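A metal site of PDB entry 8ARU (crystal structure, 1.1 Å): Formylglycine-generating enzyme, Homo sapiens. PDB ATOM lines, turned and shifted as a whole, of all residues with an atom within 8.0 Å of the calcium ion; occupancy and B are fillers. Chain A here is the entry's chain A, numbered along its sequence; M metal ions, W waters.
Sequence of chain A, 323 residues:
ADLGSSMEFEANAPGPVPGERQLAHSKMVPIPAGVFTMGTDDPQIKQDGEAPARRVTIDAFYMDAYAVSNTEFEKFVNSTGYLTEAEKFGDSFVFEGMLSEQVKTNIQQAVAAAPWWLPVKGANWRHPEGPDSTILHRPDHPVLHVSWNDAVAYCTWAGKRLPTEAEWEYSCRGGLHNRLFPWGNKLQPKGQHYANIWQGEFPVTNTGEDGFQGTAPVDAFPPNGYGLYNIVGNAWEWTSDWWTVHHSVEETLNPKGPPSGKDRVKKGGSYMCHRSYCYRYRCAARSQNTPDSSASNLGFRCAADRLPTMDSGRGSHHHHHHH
The backbone NH (N) of Asn 234 is in hydrogen-bond range of the backbone carbonyl oxygen (O) of Asn 196 (2.9 Å). N of Asp 210 lies within hydrogen-bond range of OE1 of Gln 199, 3.0 Å away. The side-chain amide nitrogen (ND2) of Asn 196 lies within hydrogen-bond range of the backbone carbonyl oxygen (O) of Gly 214. The side-chain amide nitrogen (ND2) of Asn 196 lies close to the backbone NH (N) of Ala 216 (3.4 Å).
Four residues have an atom within 4 Å of the calcium ion: Asn 196, Ile 197, Asp 210 and Phe 212.
The calcium ion is bound by the side-chain amide oxygen (OD1) of Asn 196, the backbone carbonyl oxygen (O) of Ile 197, the backbone carbonyl oxygen (O) of Phe 212, water W1, water W2, the side-chain carboxylate (OD1) of Asp 210 and the side-chain carboxylate (OD2) of Asp 210. The calcium ion has seven donor atoms within binding distance.
Water W2 lies within hydrogen-bond range of O of Gln 213 (2.6 Å), O of Tyr 271 (2.8 Å) and ND2 of Asn 206 (3.0 Å). Water W1 lies within hydrogen-bond range of OD1 of Asn 206, OE1 of Gln 199 and N of Gly 208.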
ATOM      1  N   HIS A 193     -33.538 -31.000  10.402  1.00  0.00           N
ATOM      2  CA  HIS A 193     -33.170 -29.901  11.296  1.00  0.00           C
ATOM      3  C   HIS A 193     -34.308 -29.609  12.251  1.00  0.00           C
ATOM      4  O   HIS A 193     -35.467 -29.495  11.825  1.00  0.00           O
ATOM      5  CB  HIS A 193     -32.760 -28.657  10.508  1.00  0.00           C
ATOM      6  CG  HIS A 193     -31.415 -28.797   9.906  1.00  0.00           C
ATOM      7  ND1 HIS A 193     -30.261 -28.620  10.635  1.00  0.00           N
ATOM      8  CD2 HIS A 193     -31.036 -29.177   8.664  1.00  0.00           C
ATOM      9  CE1 HIS A 193     -29.214 -28.891   9.867  1.00  0.00           C
ATOM     10  NE2 HIS A 193     -29.650 -29.217   8.665  1.00  0.00           N
ATOM     11  N   ALA A 195     -33.825 -27.098  14.861  1.00  0.00           N
ATOM     12  CA  ALA A 195     -33.611 -25.754  15.405  1.00  0.00           C
ATOM     13  C   ALA A 195     -32.742 -24.962  14.450  1.00  0.00           C
ATOM     14  O   ALA A 195     -31.975 -25.529  13.648  1.00  0.00           O
ATOM     15  CB  ALA A 195     -32.912 -25.848  16.780  1.00  0.00           C
ATOM     16  N   ASN A 196     -32.821 -23.623  14.589  1.00  0.00           N
ATOM     17  CA  ASN A 196     -32.067 -22.691  13.764  1.00  0.00           C
ATOM     18  C   ASN A 196     -30.762 -22.334  14.471  1.00  0.00           C
ATOM     19  O   ASN A 196     -30.741 -21.484  15.380  1.00  0.00           O
ATOM     20  CB  ASN A 196     -32.913 -21.461  13.521  1.00  0.00           C
ATOM     21  CG  ASN A 196     -32.183 -20.446  12.685  1.00  0.00           C
ATOM     22  OD1 ASN A 196     -31.221 -20.802  11.977  1.00  0.00           O
ATOM     23  ND2 ASN A 196     -32.635 -19.202  12.720  1.00  0.00           N
ATOM     24  N   ILE A 197     -29.672 -22.983  14.056  1.00  0.00           N
ATOM     25  CA  ILE A 197     -28.319 -22.682  14.530  1.00  0.00           C
ATOM     26  C   ILE A 197     -27.437 -22.443  13.317  1.00  0.00           C
ATOM     27  O   ILE A 197     -27.952 -22.186  12.242  1.00  0.00           O
ATOM     28  CB  ILE A 197     -27.790 -23.729  15.515  1.00  0.00           C
ATOM     29  CG1 ILE A 197     -27.719 -25.148  14.902  1.00  0.00           C
ATOM     30  CG2 ILE A 197     -28.677 -23.691  16.783  1.00  0.00           C
ATOM     31  CD1 ILE A 197     -26.978 -26.115  15.800  1.00  0.00           C
ATOM     32  N   TRP A 198     -26.116 -22.502  13.462  1.00  0.00           N
ATOM     33  CA  TRP A 198     -25.196 -22.218  12.360  1.00  0.00           C
ATOM     34  C   TRP A 198     -24.761 -23.542  11.741  1.00  0.00           C
ATOM     35  O   TRP A 198     -24.493 -24.509  12.461  1.00  0.00           O
ATOM     36  CB  TRP A 198     -23.957 -21.574  12.965  1.00  0.00           C
ATOM     37  CG  TRP A 198     -22.934 -21.061  12.020  1.00  0.00           C
ATOM     38  CD1 TRP A 198     -21.980 -21.768  11.337  1.00  0.00           C
ATOM     39  CD2 TRP A 198     -22.765 -19.692  11.612  1.00  0.00           C
ATOM     40  NE1 TRP A 198     -21.199 -20.917  10.586  1.00  0.00           N
ATOM     41  CE2 TRP A 198     -21.659 -19.627  10.726  1.00  0.00           C
ATOM     42  CE3 TRP A 198     -23.419 -18.493  11.950  1.00  0.00           C
ATOM     43  CZ2 TRP A 198     -21.183 -18.412  10.173  1.00  0.00           C
ATOM     44  CZ3 TRP A 198     -22.955 -17.282  11.398  1.00  0.00           C
ATOM     45  CH2 TRP A 198     -21.849 -17.260  10.524  1.00  0.00           C
ATOM     46  N   GLN A 199     -24.645 -23.582  10.426  1.00  0.00           N
ATOM     47  CA  GLN A 199     -23.911 -24.642   9.740  1.00  0.00           C
ATOM     48  C   GLN A 199     -22.817 -23.987   8.919  1.00  0.00           C
ATOM     49  O   GLN A 199     -23.029 -22.915   8.341  1.00  0.00           O
ATOM     50  CB  GLN A 199     -24.804 -25.498   8.839  1.00  0.00           C
ATOM     51  CG  GLN A 199     -25.897 -26.262   9.558  1.00  0.00           C
ATOM     52  CD  GLN A 199     -27.134 -25.387   9.806  1.00  0.00           C
ATOM     53  OE1 GLN A 199     -27.536 -24.632   8.904  1.00  0.00           O
ATOM     54  NE2 GLN A 199     -27.741 -25.499  10.969  1.00  0.00           N
ATOM     55  N   ASN A 206     -21.895 -19.166   6.839  1.00  0.00           N
ATOM     56  CA  ASN A 206     -23.093 -19.816   7.318  1.00  0.00           C
ATOM     57  C   ASN A 206     -23.792 -20.342   6.070  1.00  0.00           C
ATOM     58  O   ASN A 206     -24.217 -19.554   5.222  1.00  0.00           O
ATOM     59  CB  ASN A 206     -23.996 -18.822   8.048  1.00  0.00           C
ATOM     60  CG  ASN A 206     -25.178 -19.499   8.711  1.00  0.00           C
ATOM     61  OD1 ASN A 206     -25.479 -20.684   8.468  1.00  0.00           O
ATOM     62  ND2 ASN A 206     -25.874 -18.767   9.534  1.00  0.00           N
ATOM     63  N   THR A 207     -23.889 -21.667   5.956  1.00  0.00           N
ATOM     64  CA  THR A 207     -24.449 -22.221   4.731  1.00  0.00           C
ATOM     65  C   THR A 207     -25.959 -22.085   4.639  1.00  0.00           C
ATOM     66  O   THR A 207     -26.517 -22.237   3.545  1.00  0.00           O
ATOM     67  CB  THR A 207     -24.122 -23.705   4.586  1.00  0.00           C
ATOM     68  OG1 THR A 207     -24.791 -24.403   5.634  1.00  0.00           O
ATOM     69  CG2 THR A 207     -22.602 -23.924   4.619  1.00  0.00           C
ATOM     70  N   GLY A 208     -26.629 -21.823   5.759  1.00  0.00           N
ATOM     71  CA  GLY A 208     -28.076 -21.778   5.672  1.00  0.00           C
ATOM     72  C   GLY A 208     -28.739 -23.110   5.424  1.00  0.00           C
ATOM     73  O   GLY A 208     -29.881 -23.157   4.956  1.00  0.00           O
ATOM     74  N   GLU A 209     -28.043 -24.202   5.740  1.00  0.00           N
ATOM     75  CA  GLU A 209     -28.557 -25.537   5.454  1.00  0.00           C
ATOM     76  C   GLU A 209     -29.888 -25.770   6.154  1.00  0.00           C
ATOM     77  O   GLU A 209     -30.762 -26.434   5.599  1.00  0.00           O
ATOM     78  CB  GLU A 209     -27.528 -26.556   5.931  1.00  0.00           C
ATOM     79  CG  GLU A 209     -27.928 -28.000   5.732  1.00  0.00           C
ATOM     80  CD  GLU A 209     -27.040 -28.932   6.546  1.00  0.00           C
ATOM     81  OE1 GLU A 209     -25.842 -28.613   6.753  1.00  0.00           O
ATOM     82  OE2 GLU A 209     -27.532 -30.020   6.907  1.00  0.00           O
ATOM     83  N   ASP A 210     -30.075 -25.217   7.366  1.00  0.00           N
ATOM     84  CA  ASP A 210     -31.328 -25.430   8.096  1.00  0.00           C
ATOM     85  C   ASP A 210     -32.476 -24.545   7.599  1.00  0.00           C
ATOM     86  O   ASP A 210     -33.573 -24.597   8.174  1.00  0.00           O
ATOM     87  CB  ASP A 210     -31.096 -25.307   9.605  1.00  0.00           C
ATOM     88  CG  ASP A 210     -30.646 -23.913  10.025  1.00  0.00           C
ATOM     89  OD1 ASP A 210     -30.864 -22.945   9.270  1.00  0.00           O
ATOM     90  OD2 ASP A 210     -30.082 -23.798  11.124  1.00  0.00           O
ATOM     91  N   GLY A 211     -32.249 -23.723   6.571  1.00  0.00           N
ATOM     92  CA  GLY A 211     -33.268 -22.878   6.006  1.00  0.00           C
ATOM     93  C   GLY A 211     -33.170 -21.414   6.380  1.00  0.00           C
ATOM     94  O   GLY A 211     -33.934 -20.629   5.811  1.00  0.00           O
ATOM     95  N   PHE A 212     -32.286 -21.031   7.311  1.00  0.00           N
ATOM     96  CA  PHE A 212     -32.260 -19.652   7.815  1.00  0.00           C
ATOM     97  C   PHE A 212     -30.825 -19.253   8.163  1.00  0.00           C
ATOM     98  O   PHE A 212     -30.178 -19.934   8.966  1.00  0.00           O
ATOM     99  CB  PHE A 212     -33.166 -19.484   9.054  1.00  0.00           C
ATOM    100  CG  PHE A 212     -34.578 -19.870   8.780  1.00  0.00           C
ATOM    101  CD1 PHE A 212     -35.469 -18.960   8.215  1.00  0.00           C
ATOM    102  CD2 PHE A 212     -34.991 -21.209   8.999  1.00  0.00           C
ATOM    103  CE1 PHE A 212     -36.766 -19.348   7.862  1.00  0.00           C
ATOM    104  CE2 PHE A 212     -36.290 -21.608   8.665  1.00  0.00           C
ATOM    105  CZ  PHE A 212     -37.170 -20.679   8.050  1.00  0.00           C
ATOM    106  N   GLN A 213     -30.351 -18.194   7.526  1.00  0.00           N
ATOM    107  CA  GLN A 213     -29.106 -17.536   7.878  1.00  0.00           C
ATOM    108  C   GLN A 213     -29.236 -16.801   9.221  1.00  0.00           C
ATOM    109  O   GLN A 213     -28.614 -17.182  10.218  1.00  0.00           O
ATOM    110  CB  GLN A 213     -28.705 -16.570   6.755  1.00  0.00           C
ATOM    111  CG  GLN A 213     -28.244 -17.288   5.482  1.00  0.00           C
ATOM    112  CD  GLN A 213     -26.803 -17.720   5.552  1.00  0.00           C
ATOM    113  OE1 GLN A 213     -26.063 -17.262   6.419  1.00  0.00           O
ATOM    114  NE2 GLN A 213     -26.377 -18.597   4.646  1.00  0.00           N
ATOM    115  N   GLY A 214     -30.081 -15.764   9.255  1.00  0.00           N
ATOM    116  CA  GLY A 214     -30.418 -15.026  10.458  1.00  0.00           C
ATOM    117  C   GLY A 214     -31.530 -15.759  11.173  1.00  0.00           C
ATOM    118  O   GLY A 214     -31.604 -17.000  11.176  1.00  0.00           O
ATOM    119  N   THR A 215     -32.411 -15.012  11.825  1.00  0.00           N
ATOM    120  CA  THR A 215     -33.525 -15.636  12.537  1.00  0.00           C
ATOM    121  C   THR A 215     -34.506 -16.282  11.575  1.00  0.00           C
ATOM    122  O   THR A 215     -34.555 -15.987  10.376  1.00  0.00           O
ATOM    123  CB  THR A 215     -34.299 -14.566  13.351  1.00  0.00           C
ATOM    124  OG1 THR A 215     -34.741 -13.501  12.490  1.00  0.00           O
ATOM    125  CG2 THR A 215     -33.421 -14.037  14.484  1.00  0.00           C
ATOM    126  N   ALA A 216     -35.329 -17.137  12.141  1.00  0.00           N
ATOM    127  CA  ALA A 216     -36.480 -17.744  11.500  1.00  0.00           C
ATOM    128  C   ALA A 216     -37.757 -17.220  12.135  1.00  0.00           C
ATOM    129  O   ALA A 216     -37.736 -16.756  13.283  1.00  0.00           O
ATOM    130  CB  ALA A 216     -36.418 -19.256  11.699  1.00  0.00           C
ATOM    131  N   PHE A 221     -39.863 -24.722  12.651  1.00  0.00           N
ATOM    132  CA  PHE A 221     -39.285 -25.952  13.228  1.00  0.00           C
ATOM    133  C   PHE A 221     -40.300 -26.699  14.065  1.00  0.00           C
ATOM    134  O   PHE A 221     -41.361 -26.167  14.407  1.00  0.00           O
ATOM    135  CB  PHE A 221     -37.935 -25.695  13.947  1.00  0.00           C
ATOM    136  CG  PHE A 221     -36.869 -25.221  12.989  1.00  0.00           C
ATOM    137  CD1 PHE A 221     -36.186 -26.124  12.166  1.00  0.00           C
ATOM    138  CD2 PHE A 221     -36.563 -23.855  12.875  1.00  0.00           C
ATOM    139  CE1 PHE A 221     -35.224 -25.647  11.251  1.00  0.00           C
ATOM    140  CE2 PHE A 221     -35.649 -23.394  11.940  1.00  0.00           C
ATOM    141  CZ  PHE A 221     -34.963 -24.304  11.130  1.00  0.00           C
ATOM    142  N   ASN A 234     -32.291 -20.028  17.288  1.00  0.00           N
ATOM    143  CA  ASN A 234     -33.028 -18.857  16.811  1.00  0.00           C
ATOM    144  C   ASN A 234     -32.494 -17.582  17.467  1.00  0.00           C
ATOM    145  O   ASN A 234     -31.700 -16.868  16.839  1.00  0.00           O
ATOM    146  CB  ASN A 234     -34.560 -19.012  16.841  1.00  0.00           C
ATOM    147  CG  ASN A 234     -35.227 -18.340  15.643  1.00  0.00           C
ATOM    148  OD1 ASN A 234     -34.590 -18.157  14.603  1.00  0.00           O
ATOM    149  ND2 ASN A 234     -36.493 -17.932  15.776  1.00  0.00           N
ATOM    150  N   SER A 270     -28.644 -19.344  19.877  1.00  0.00           N
ATOM    151  CA  SER A 270     -29.156 -18.531  18.789  1.00  0.00           C
ATOM    152  C   SER A 270     -28.786 -19.122  17.431  1.00  0.00           C
ATOM    153  O   SER A 270     -28.077 -20.130  17.333  1.00  0.00           O
ATOM    154  CB  SER A 270     -28.656 -17.079  18.862  1.00  0.00           C
ATOM    155  OG  SER A 270     -27.318 -17.002  18.399  1.00  0.00           O
ATOM    156  N   TYR A 271     -29.221 -18.412  16.379  1.00  0.00           N
ATOM    157  CA  TYR A 271     -28.862 -18.763  15.012  1.00  0.00           C
ATOM    158  C   TYR A 271     -27.360 -18.726  14.730  1.00  0.00           C
ATOM    159  O   TYR A 271     -26.924 -19.282  13.704  1.00  0.00           O
ATOM    160  CB  TYR A 271     -29.601 -17.847  14.016  1.00  0.00           C
ATOM    161  CG  TYR A 271     -29.118 -16.397  13.955  1.00  0.00           C
ATOM    162  CD1 TYR A 271     -27.995 -16.053  13.217  1.00  0.00           C
ATOM    163  CD2 TYR A 271     -29.801 -15.376  14.633  1.00  0.00           C
ATOM    164  CE1 TYR A 271     -27.552 -14.755  13.108  1.00  0.00           C
ATOM    165  CE2 TYR A 271     -29.395 -14.056  14.528  1.00  0.00           C
ATOM    166  CZ  TYR A 271     -28.276 -13.753  13.755  1.00  0.00           C
ATOM    167  OH  TYR A 271     -27.834 -12.461  13.595  1.00  0.00           O
ATOM    168  N   MET A 272     -26.577 -18.114  15.621  1.00  0.00           N
ATOM    169  CA  MET A 272     -25.130 -18.038  15.493  1.00  0.00           C
ATOM    170  C   MET A 272     -24.399 -19.270  15.991  1.00  0.00           C
ATOM    171  O   MET A 272     -23.188 -19.424  15.738  1.00  0.00           O
ATOM    172  CB  MET A 272     -24.579 -16.832  16.239  1.00  0.00           C
ATOM    173  CG  MET A 272     -25.076 -15.525  15.696  1.00  0.00           C
ATOM    174  SD  MET A 272     -24.613 -14.120  16.714  1.00  0.00           S
ATOM    175  CE  MET A 272     -22.833 -14.156  16.674  1.00  0.00           C
ATOM    176  N   CYS A 273     -25.048 -20.149  16.759  1.00  0.00           N
ATOM    177  CA  CYS A 273     -24.282 -21.089  17.519  1.00  0.00           C
ATOM    178  C   CYS A 273     -23.844 -22.299  16.681  1.00  0.00           C
ATOM    179  O   CYS A 273     -24.612 -22.826  15.900  1.00  0.00           O
ATOM    180  CB  CYS A 273     -25.097 -21.514  18.720  1.00  0.00           C
ATOM    181  SG  CYS A 273     -24.144 -22.369  19.853  1.00  0.00           S
HETATM  182 CA    CA M   1     -29.477 -21.436  10.638  1.00  0.00          CA
HETATM  183  O   HOH W   1     -27.767 -21.945   9.061  1.00  0.00           O
HETATM  184  O   HOH W   2     -28.198 -19.507  11.206  1.00  0.00           O
